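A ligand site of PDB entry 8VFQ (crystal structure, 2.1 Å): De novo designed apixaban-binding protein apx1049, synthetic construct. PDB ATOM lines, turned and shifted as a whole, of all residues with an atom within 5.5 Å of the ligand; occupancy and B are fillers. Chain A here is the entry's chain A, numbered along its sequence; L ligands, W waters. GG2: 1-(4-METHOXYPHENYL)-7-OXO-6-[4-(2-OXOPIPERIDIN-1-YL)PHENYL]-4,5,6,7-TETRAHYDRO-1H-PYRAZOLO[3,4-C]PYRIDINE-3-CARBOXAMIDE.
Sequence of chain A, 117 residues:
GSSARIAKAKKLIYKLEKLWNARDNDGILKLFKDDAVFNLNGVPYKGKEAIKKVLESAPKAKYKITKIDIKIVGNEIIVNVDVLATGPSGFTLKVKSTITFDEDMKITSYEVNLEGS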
ATOM      1  N   ILE A  13     -21.666  15.429  -3.330  1.00  0.00           N
ATOM      2  CA  ILE A  13     -21.750  14.216  -2.524  1.00  0.00           C
ATOM      3  C   ILE A  13     -21.135  14.449  -1.149  1.00  0.00           C
ATOM      4  O   ILE A  13     -21.715  14.104  -0.122  1.00  0.00           O
ATOM      5  CB  ILE A  13     -21.087  13.028  -3.235  1.00  0.00           C
ATOM      6  CG1 ILE A  13     -21.832  12.680  -4.525  1.00  0.00           C
ATOM      7  CG2 ILE A  13     -21.034  11.822  -2.306  1.00  0.00           C
ATOM      8  CD1 ILE A  13     -23.143  11.961  -4.302  1.00  0.00           C
ATOM      9  N   LEU A  16     -23.263  16.404   0.796  1.00  0.00           N
ATOM     10  CA  LEU A  16     -24.364  15.604   1.320  1.00  0.00           C
ATOM     11  C   LEU A  16     -23.954  14.802   2.541  1.00  0.00           C
ATOM     12  O   LEU A  16     -24.787  14.578   3.428  1.00  0.00           O
ATOM     13  CB  LEU A  16     -24.909  14.683   0.223  1.00  0.00           C
ATOM     14  CG  LEU A  16     -26.168  15.166  -0.499  1.00  0.00           C
ATOM     15  CD1 LEU A  16     -26.642  14.127  -1.504  1.00  0.00           C
ATOM     16  CD2 LEU A  16     -27.258  15.507   0.498  1.00  0.00           C
ATOM     17  N   GLU A  17     -22.699  14.367   2.622  1.00  0.00           N
ATOM     18  CA  GLU A  17     -22.247  13.622   3.794  1.00  0.00           C
ATOM     19  C   GLU A  17     -22.345  14.480   5.049  1.00  0.00           C
ATOM     20  O   GLU A  17     -22.855  14.037   6.086  1.00  0.00           O
ATOM     21  CB  GLU A  17     -20.816  13.114   3.593  1.00  0.00           C
ATOM     22  CG  GLU A  17     -20.231  12.414   4.815  1.00  0.00           C
ATOM     23  CD  GLU A  17     -18.744  12.122   4.674  1.00  0.00           C
ATOM     24  OE1 GLU A  17     -17.942  13.051   4.858  1.00  0.00           O
ATOM     25  OE2 GLU A  17     -18.385  10.966   4.373  1.00  0.00           O
ATOM     26  N   TRP A  20     -25.988  14.990   5.993  1.00  0.00           N
ATOM     27  CA  TRP A  20     -26.628  13.841   6.631  1.00  0.00           C
ATOM     28  C   TRP A  20     -26.187  13.696   8.083  1.00  0.00           C
ATOM     29  O   TRP A  20     -26.995  13.341   8.949  1.00  0.00           O
ATOM     30  CB  TRP A  20     -26.304  12.568   5.850  1.00  0.00           C
ATOM     31  CG  TRP A  20     -27.247  12.297   4.733  1.00  0.00           C
ATOM     32  CD1 TRP A  20     -27.031  12.523   3.412  1.00  0.00           C
ATOM     33  CD2 TRP A  20     -28.560  11.744   4.839  1.00  0.00           C
ATOM     34  NE1 TRP A  20     -28.123  12.147   2.683  1.00  0.00           N
ATOM     35  CE2 TRP A  20     -29.082  11.658   3.535  1.00  0.00           C
ATOM     36  CE3 TRP A  20     -29.345  11.310   5.913  1.00  0.00           C
ATOM     37  CZ2 TRP A  20     -30.354  11.168   3.267  1.00  0.00           C
ATOM     38  CZ3 TRP A  20     -30.604  10.819   5.641  1.00  0.00           C
ATOM     39  CH2 TRP A  20     -31.096  10.745   4.337  1.00  0.00           C
ATOM     40  N   PHE A  38     -37.148   9.540  -3.484  1.00  0.00           N
ATOM     41  CA  PHE A  38     -36.190   8.943  -2.552  1.00  0.00           C
ATOM     42  C   PHE A  38     -36.561   7.465  -2.457  1.00  0.00           C
ATOM     43  O   PHE A  38     -37.549   7.097  -1.812  1.00  0.00           O
ATOM     44  CB  PHE A  38     -36.231   9.632  -1.195  1.00  0.00           C
ATOM     45  CG  PHE A  38     -35.162   9.166  -0.229  1.00  0.00           C
ATOM     46  CD1 PHE A  38     -35.185   7.883   0.300  1.00  0.00           C
ATOM     47  CD2 PHE A  38     -34.125  10.009   0.130  1.00  0.00           C
ATOM     48  CE1 PHE A  38     -34.197   7.464   1.171  1.00  0.00           C
ATOM     49  CE2 PHE A  38     -33.136   9.586   1.010  1.00  0.00           C
ATOM     50  CZ  PHE A  38     -33.177   8.313   1.526  1.00  0.00           C
ATOM     51  N   LEU A  40     -36.053   4.448  -0.791  1.00  0.00           N
ATOM     52  CA  LEU A  40     -35.539   3.906   0.467  1.00  0.00           C
ATOM     53  C   LEU A  40     -35.741   2.390   0.464  1.00  0.00           C
ATOM     54  O   LEU A  40     -36.831   1.897   0.760  1.00  0.00           O
ATOM     55  CB  LEU A  40     -36.237   4.556   1.659  1.00  0.00           C
ATOM     56  CG  LEU A  40     -35.929   3.961   3.031  1.00  0.00           C
ATOM     57  CD1 LEU A  40     -34.427   3.952   3.291  1.00  0.00           C
ATOM     58  CD2 LEU A  40     -36.655   4.722   4.128  1.00  0.00           C
ATOM     59  N   VAL A  54     -38.889  11.009   5.151  1.00  0.00           N
ATOM     60  CA  VAL A  54     -37.804  10.032   5.112  1.00  0.00           C
ATOM     61  C   VAL A  54     -36.575  10.563   5.835  1.00  0.00           C
ATOM     62  O   VAL A  54     -35.902   9.836   6.576  1.00  0.00           O
ATOM     63  CB  VAL A  54     -37.489   9.657   3.652  1.00  0.00           C
ATOM     64  CG1 VAL A  54     -36.102   9.051   3.547  1.00  0.00           C
ATOM     65  CG2 VAL A  54     -38.538   8.703   3.105  1.00  0.00           C
ATOM     66  N   SER A  57     -37.313  10.471   9.727  1.00  0.00           N
ATOM     67  CA  SER A  57     -37.420   9.123  10.287  1.00  0.00           C
ATOM     68  C   SER A  57     -36.127   8.334  10.196  1.00  0.00           C
ATOM     69  O   SER A  57     -36.079   7.202  10.687  1.00  0.00           O
ATOM     70  CB  SER A  57     -38.538   8.349   9.588  1.00  0.00           C
ATOM     71  OG  SER A  57     -39.817   8.831   9.972  1.00  0.00           O
ATOM     72  N   ALA A  58     -35.082   8.887   9.594  1.00  0.00           N
ATOM     73  CA  ALA A  58     -33.817   8.190   9.491  1.00  0.00           C
ATOM     74  C   ALA A  58     -33.206   7.999  10.876  1.00  0.00           C
ATOM     75  O   ALA A  58     -33.423   8.809  11.781  1.00  0.00           O
ATOM     76  CB  ALA A  58     -32.850   8.968   8.589  1.00  0.00           C
ATOM     77  N   PRO A  59     -32.435   6.935  11.075  1.00  0.00           N
ATOM     78  CA  PRO A  59     -31.764   6.736  12.358  1.00  0.00           C
ATOM     79  C   PRO A  59     -30.693   7.801  12.587  1.00  0.00           C
ATOM     80  O   PRO A  59     -30.250   8.480  11.664  1.00  0.00           O
ATOM     81  CB  PRO A  59     -31.138   5.344  12.246  1.00  0.00           C
ATOM     82  CG  PRO A  59     -31.823   4.701  11.068  1.00  0.00           C
ATOM     83  CD  PRO A  59     -32.186   5.814  10.151  1.00  0.00           C
ATOM     84  N   ALA A  61     -27.532   8.297  12.595  1.00  0.00           N
ATOM     85  CA  ALA A  61     -26.380   7.599  12.051  1.00  0.00           C
ATOM     86  C   ALA A  61     -25.231   8.555  11.755  1.00  0.00           C
ATOM     87  O   ALA A  61     -25.427   9.766  11.590  1.00  0.00           O
ATOM     88  CB  ALA A  61     -26.762   6.838  10.769  1.00  0.00           C
ATOM     89  N   TYR A  63     -22.163   8.720   8.880  1.00  0.00           N
ATOM     90  CA  TYR A  63     -21.850   8.178   7.574  1.00  0.00           C
ATOM     91  C   TYR A  63     -20.438   8.563   7.162  1.00  0.00           C
ATOM     92  O   TYR A  63     -20.004   9.696   7.386  1.00  0.00           O
ATOM     93  CB  TYR A  63     -22.841   8.678   6.514  1.00  0.00           C
ATOM     94  CG  TYR A  63     -24.293   8.431   6.860  1.00  0.00           C
ATOM     95  CD1 TYR A  63     -24.835   7.152   6.804  1.00  0.00           C
ATOM     96  CD2 TYR A  63     -25.126   9.482   7.243  1.00  0.00           C
ATOM     97  CE1 TYR A  63     -26.162   6.929   7.121  1.00  0.00           C
ATOM     98  CE2 TYR A  63     -26.454   9.263   7.551  1.00  0.00           C
ATOM     99  CZ  TYR A  63     -26.970   7.983   7.487  1.00  0.00           C
ATOM    100  OH  TYR A  63     -28.298   7.747   7.798  1.00  0.00           O
ATOM    101  N   ILE A  65     -18.090   8.187   3.551  1.00  0.00           N
ATOM    102  CA  ILE A  65     -17.939   7.726   2.178  1.00  0.00           C
ATOM    103  C   ILE A  65     -16.655   6.922   2.057  1.00  0.00           C
ATOM    104  O   ILE A  65     -15.605   7.294   2.607  1.00  0.00           O
ATOM    105  CB  ILE A  65     -17.939   8.919   1.205  1.00  0.00           C
ATOM    106  CG1 ILE A  65     -19.232   9.715   1.347  1.00  0.00           C
ATOM    107  CG2 ILE A  65     -17.738   8.439  -0.227  1.00  0.00           C
ATOM    108  CD1 ILE A  65     -19.075  11.183   1.005  1.00  0.00           C
ATOM    109  N   VAL A  81     -22.259   5.616  -4.617  1.00  0.00           N
ATOM    110  CA  VAL A  81     -21.403   5.931  -3.478  1.00  0.00           C
ATOM    111  C   VAL A  81     -21.502   4.811  -2.452  1.00  0.00           C
ATOM    112  O   VAL A  81     -22.610   4.465  -2.011  1.00  0.00           O
ATOM    113  CB  VAL A  81     -21.756   7.296  -2.849  1.00  0.00           C
ATOM    114  CG1 VAL A  81     -23.264   7.437  -2.670  1.00  0.00           C
ATOM    115  CG2 VAL A  81     -21.050   7.468  -1.530  1.00  0.00           C
ATOM    116  N   VAL A  83     -20.903   3.752   1.333  1.00  0.00           N
ATOM    117  CA  VAL A  83     -20.990   4.514   2.566  1.00  0.00           C
ATOM    118  C   VAL A  83     -20.868   3.567   3.752  1.00  0.00           C
ATOM    119  O   VAL A  83     -21.541   2.530   3.793  1.00  0.00           O
ATOM    120  CB  VAL A  83     -22.312   5.309   2.656  1.00  0.00           C
ATOM    121  CG1 VAL A  83     -22.464   5.943   4.022  1.00  0.00           C
ATOM    122  CG2 VAL A  83     -22.383   6.354   1.559  1.00  0.00           C
ATOM    123  N   ALA A  85     -22.085   3.249   7.225  1.00  0.00           N
ATOM    124  CA  ALA A  85     -23.130   3.782   8.084  1.00  0.00           C
ATOM    125  C   ALA A  85     -22.919   3.245   9.490  1.00  0.00           C
ATOM    126  O   ALA A  85     -23.006   2.030   9.721  1.00  0.00           O
ATOM    127  CB  ALA A  85     -24.514   3.422   7.542  1.00  0.00           C
ATOM    128  N   THR A  86     -22.632   4.144  10.428  1.00  0.00           N
ATOM    129  CA  THR A  86     -22.477   3.801  11.838  1.00  0.00           C
ATOM    130  C   THR A  86     -23.736   4.246  12.572  1.00  0.00           C
ATOM    131  O   THR A  86     -24.123   5.424  12.495  1.00  0.00           O
ATOM    132  CB  THR A  86     -21.243   4.473  12.441  1.00  0.00           C
ATOM    133  OG1 THR A  86     -20.089   4.151  11.649  1.00  0.00           O
ATOM    134  CG2 THR A  86     -21.014   3.995  13.851  1.00  0.00           C
ATOM    135  N   GLY A  87     -24.386   3.319  13.267  1.00  0.00           N
ATOM    136  CA  GLY A  87     -25.651   3.606  13.901  1.00  0.00           C
ATOM    137  C   GLY A  87     -25.498   4.175  15.296  1.00  0.00           C
ATOM    138  O   GLY A  87     -24.388   4.372  15.803  1.00  0.00           O
ATOM    139  N   PHE A  91     -23.007   0.045  15.643  1.00  0.00           N
ATOM    140  CA  PHE A  91     -23.007  -0.965  14.596  1.00  0.00           C
ATOM    141  C   PHE A  91     -22.735  -0.313  13.241  1.00  0.00           C
ATOM    142  O   PHE A  91     -23.513   0.527  12.789  1.00  0.00           O
ATOM    143  CB  PHE A  91     -24.323  -1.746  14.597  1.00  0.00           C
ATOM    144  CG  PHE A  91     -25.497  -0.987  15.158  1.00  0.00           C
ATOM    145  CD1 PHE A  91     -26.063   0.076  14.474  1.00  0.00           C
ATOM    146  CD2 PHE A  91     -26.047  -1.349  16.379  1.00  0.00           C
ATOM    147  CE1 PHE A  91     -27.148   0.759  14.994  1.00  0.00           C
ATOM    148  CE2 PHE A  91     -27.133  -0.666  16.899  1.00  0.00           C
ATOM    149  CZ  PHE A  91     -27.680   0.391  16.207  1.00  0.00           C
ATOM    150  N   THR A  92     -21.629  -0.708  12.609  1.00  0.00           N
ATOM    151  CA  THR A  92     -21.231  -0.142  11.328  1.00  0.00           C
ATOM    152  C   THR A  92     -21.748  -1.047  10.221  1.00  0.00           C
ATOM    153  O   THR A  92     -21.532  -2.270  10.245  1.00  0.00           O
ATOM    154  CB  THR A  92     -19.708  -0.015  11.237  1.00  0.00           C
ATOM    155  OG1 THR A  92     -19.094  -1.231  11.695  1.00  0.00           O
ATOM    156  CG2 THR A  92     -19.228   1.128  12.112  1.00  0.00           C
ATOM    157  N   LEU A  93     -22.441  -0.460   9.242  1.00  0.00           N
ATOM    158  CA  LEU A  93     -23.065  -1.230   8.178  1.00  0.00           C
ATOM    159  C   LEU A  93     -22.710  -0.607   6.834  1.00  0.00           C
ATOM    160  O   LEU A  93     -22.757   0.619   6.678  1.00  0.00           O
ATOM    161  CB  LEU A  93     -24.576  -1.288   8.352  1.00  0.00           C
ATOM    162  CG  LEU A  93     -25.283  -2.506   7.737  1.00  0.00           C
ATOM    163  CD1 LEU A  93     -25.026  -3.748   8.584  1.00  0.00           C
ATOM    164  CD2 LEU A  93     -26.771  -2.233   7.586  1.00  0.00           C
ATOM    165  N   VAL A  95     -23.563   0.502   3.375  1.00  0.00           N
ATOM    166  CA  VAL A  95     -24.757   0.869   2.618  1.00  0.00           C
ATOM    167  C   VAL A  95     -24.318   1.475   1.291  1.00  0.00           C
ATOM    168  O   VAL A  95     -23.141   1.747   1.062  1.00  0.00           O
ATOM    169  CB  VAL A  95     -25.667   1.832   3.405  1.00  0.00           C
ATOM    170  CG1 VAL A  95     -25.801   1.382   4.850  1.00  0.00           C
ATOM    171  CG2 VAL A  95     -25.145   3.252   3.334  1.00  0.00           C
ATOM    172  N   SER A  97     -25.763   4.176  -2.080  1.00  0.00           N
ATOM    173  CA  SER A  97     -26.715   5.133  -2.600  1.00  0.00           C
ATOM    174  C   SER A  97     -26.492   5.302  -4.096  1.00  0.00           C
ATOM    175  O   SER A  97     -25.350   5.300  -4.564  1.00  0.00           O
ATOM    176  CB  SER A  97     -26.592   6.495  -1.891  1.00  0.00           C
ATOM    177  OG  SER A  97     -26.798   6.359  -0.498  1.00  0.00           O
ATOM    178  N   ILE A  99     -27.494   8.108  -6.674  1.00  0.00           N
ATOM    179  CA  ILE A  99     -28.013   9.468  -6.757  1.00  0.00           C
ATOM    180  C   ILE A  99     -27.885   9.942  -8.199  1.00  0.00           C
ATOM    181  O   ILE A  99     -26.790   9.909  -8.779  1.00  0.00           O
ATOM    182  CB  ILE A  99     -27.281  10.399  -5.782  1.00  0.00           C
ATOM    183  CG1 ILE A  99     -27.269   9.777  -4.387  1.00  0.00           C
ATOM    184  CG2 ILE A  99     -27.935  11.767  -5.769  1.00  0.00           C
ATOM    185  CD1 ILE A  99     -26.197  10.324  -3.464  1.00  0.00           C
ATOM    186  N   TYR A 110     -32.859   9.280  -5.735  1.00  0.00           N
ATOM    187  CA  TYR A 110     -31.937   9.015  -4.620  1.00  0.00           C
ATOM    188  C   TYR A 110     -32.296   7.650  -4.043  1.00  0.00           C
ATOM    189  O   TYR A 110     -33.104   7.553  -3.114  1.00  0.00           O
ATOM    190  CB  TYR A 110     -32.037  10.131  -3.584  1.00  0.00           C
ATOM    191  CG  TYR A 110     -30.825  10.267  -2.667  1.00  0.00           C
ATOM    192  CD1 TYR A 110     -30.340   9.185  -1.950  1.00  0.00           C
ATOM    193  CD2 TYR A 110     -30.195  11.491  -2.522  1.00  0.00           C
ATOM    194  CE1 TYR A 110     -29.244   9.325  -1.109  1.00  0.00           C
ATOM    195  CE2 TYR A 110     -29.102  11.636  -1.689  1.00  0.00           C
ATOM    196  CZ  TYR A 110     -28.626  10.553  -0.982  1.00  0.00           C
ATOM    197  OH  TYR A 110     -27.534  10.720  -0.159  1.00  0.00           O
ATOM    198  N   VAL A 112     -31.359   4.394  -1.866  1.00  0.00           N
ATOM    199  CA  VAL A 112     -30.497   3.866  -0.814  1.00  0.00           C
ATOM    200  C   VAL A 112     -30.865   2.409  -0.603  1.00  0.00           C
ATOM    201  O   VAL A 112     -32.032   2.095  -0.328  1.00  0.00           O
ATOM    202  CB  VAL A 112     -30.600   4.671   0.483  1.00  0.00           C
ATOM    203  CG1 VAL A 112     -29.874   5.998   0.346  1.00  0.00           C
ATOM    204  CG2 VAL A 112     -32.042   4.916   0.856  1.00  0.00           C
ATOM    205  N   LEU A 114     -29.910  -1.301   1.351  1.00  0.00           N
ATOM    206  CA  LEU A 114     -29.279  -1.836   2.550  1.00  0.00           C
ATOM    207  C   LEU A 114     -29.239  -3.360   2.471  1.00  0.00           C
ATOM    208  O   LEU A 114     -29.364  -3.935   1.394  1.00  0.00           O
ATOM    209  CB  LEU A 114     -30.039  -1.370   3.794  1.00  0.00           C
ATOM    210  CG  LEU A 114     -30.452   0.102   3.782  1.00  0.00           C
ATOM    211  CD1 LEU A 114     -31.354   0.455   4.952  1.00  0.00           C
ATOM    212  CD2 LEU A 114     -29.218   0.995   3.781  1.00  0.00           C
HETATM  213  C1  GG2 L   1     -27.696   1.682   9.303  1.00  0.00           C
HETATM  214  C2  GG2 L   1     -28.726   1.038   8.632  1.00  0.00           C
HETATM  215  C3  GG2 L   1     -29.702   1.782   7.987  1.00  0.00           C
HETATM  216  O4  GG2 L   1     -26.715   0.914   9.946  1.00  0.00           O
HETATM  217  N6  GG2 L   1     -31.901   3.832   7.670  1.00  0.00           N
HETATM  218  C7  GG2 L   1     -28.195   7.147   4.154  1.00  0.00           C
HETATM  219  C8  GG2 L   1     -29.234   5.348   5.627  1.00  0.00           C
HETATM  220  C10 GG2 L   1     -32.552   4.655   6.907  1.00  0.00           C
HETATM  221  C11 GG2 L   1     -34.060   4.847   6.938  1.00  0.00           C
HETATM  222  C12 GG2 L   1     -31.659   5.411   5.952  1.00  0.00           C
HETATM  223  C13 GG2 L   1     -30.431   4.854   6.359  1.00  0.00           C
HETATM  224  C14 GG2 L   1     -26.879   9.087   3.641  1.00  0.00           C
HETATM  225  C15 GG2 L   1     -25.929   1.633  10.860  1.00  0.00           C
HETATM  226  C16 GG2 L   1     -26.035   8.295   2.874  1.00  0.00           C
HETATM  227  C19 GG2 L   1     -24.978   9.216   0.798  1.00  0.00           C
HETATM  228  C20 GG2 L   1     -23.714   9.236   2.973  1.00  0.00           C
HETATM  229  C21 GG2 L   1     -23.054  10.527   2.491  1.00  0.00           C
HETATM  230  C22 GG2 L   1     -27.355   6.366   3.370  1.00  0.00           C
HETATM  231  C24 GG2 L   1     -30.630   7.352   4.818  1.00  0.00           C
HETATM  232  C4  GG2 L   1     -29.644   3.165   8.021  1.00  0.00           C
HETATM  233  C5  GG2 L   1     -28.613   3.808   8.692  1.00  0.00           C
HETATM  234  C6  GG2 L   1     -27.638   3.064   9.337  1.00  0.00           C
HETATM  235  N1  GG2 L   1     -30.666   3.942   7.359  1.00  0.00           N
HETATM  236  N5  GG2 L   1     -29.346   6.570   4.828  1.00  0.00           N
HETATM  237  C44 GG2 L   1     -27.959   8.504   4.282  1.00  0.00           C
HETATM  238  N2  GG2 L   1     -24.908   8.921   2.210  1.00  0.00           N
HETATM  239  C18 GG2 L   1     -26.273   6.944   2.737  1.00  0.00           C
HETATM  240  O3  GG2 L   1     -28.027   4.643   5.687  1.00  0.00           O
HETATM  241  C25 GG2 L   1     -23.065  10.862   0.994  1.00  0.00           C
HETATM  242  O2  GG2 L   1     -25.956   8.947   0.195  1.00  0.00           O
HETATM  243  C23 GG2 L   1     -23.784   9.860   0.105  1.00  0.00           C
HETATM  244  O1  GG2 L   1     -34.544   5.819   6.465  1.00  0.00           O
HETATM  245  N3  GG2 L   1     -34.899   3.851   7.571  1.00  0.00           N
HETATM  246  C17 GG2 L   1     -31.909   6.452   4.897  1.00  0.00           C
HETATM  247  O   HOH W   1     -36.650   7.365   7.144  1.00  0.00           O
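The side-chain hydroxyl (OH) of Tyr 63 lies close to a nitrogen (N5) of the ligand (3.4 Å).
Ile 13 touches the ligand.
Glu 17 touches the ligand (CA to C21, 3.5 Å).
CD2 of Trp 20 touches C44 of the ligand, at 3.3 Å.
CD2 of Leu 40 touches O1 of the ligand, 3.3 Å away.
Ala 58 touches the ligand.
CD of Pro 59 touches N6 of the ligand (3.2 Å).
Val 81 touches the ligand.
CG2 of Val 83 touches C20 of the ligand (3.5 Å).
O of Ala 85 touches C15 of the ligand, at 3.2 Å.
Thr 86 touches the ligand (C to C15, 3.8 Å).
Gly 87 touches the ligand (N to C15, 3.3 Å).
Phe 91 touches the ligand (O to C15, 3.3 Å).
Leu 93 touches the ligand.
Val 95 touches the ligand (CG2 to C22, 3.8 Å).
CD1 of Ile 99 touches O2 of the ligand, 3.9 Å away.
Val 112 touches the ligand (CG1 to C22, 3.95 Å).
Leu 114 touches the ligand (CD1 to C3, 3.7 Å).
20 residues have an atom within 4 Å of the ligand: Ile 13, Glu 17, Trp 20, Leu 40, Ala 58, Pro 59, Tyr 63, Val 81, Val 83, Ala 85, Thr 86, Gly 87, Phe 91, Leu 93, Val 95, Ser 97, Ile 99, Tyr 110, Val 112 and Leu 114.
The indole nitrogen (NE1) of Trp 20 sits at hydrogen-bond distance from the side-chain hydroxyl (OH) of Tyr 110, 3.2 Å away.
The backbone carbonyl oxygen (O) of Ser 97 is in hydrogen-bond range of the backbone NH (N) of Val 81.
The backbone carbonyl oxygen (O) of Ala 85 lies within hydrogen-bond range of the backbone NH (N) of Leu 93 (2.6 Å).
The side-chain carboxylate (OE2) of Glu 17 is in hydrogen-bond range of the backbone NH (N) of Ile 65, at 2.9 Å.
The backbone NH of Val 95 sits at hydrogen-bond distance from the backbone carbonyl oxygen of Val 83 (2.9 Å).
The side-chain hydroxyl (OH) of Tyr 110 lies within hydrogen-bond range of an oxygen (O2) of the ligand (2.4 Å).
The side-chain hydroxyl of Ser 97 sits at hydrogen-bond distance from an oxygen (O2) of the ligand, at 2.8 Å.
Water W1 lies within hydrogen-bond range of the backbone carbonyl oxygen of Val 54 (2.6 Å), an oxygen (O1) of the ligand (2.7 Å) and the backbone NH of Ala 58 (3.3 Å).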
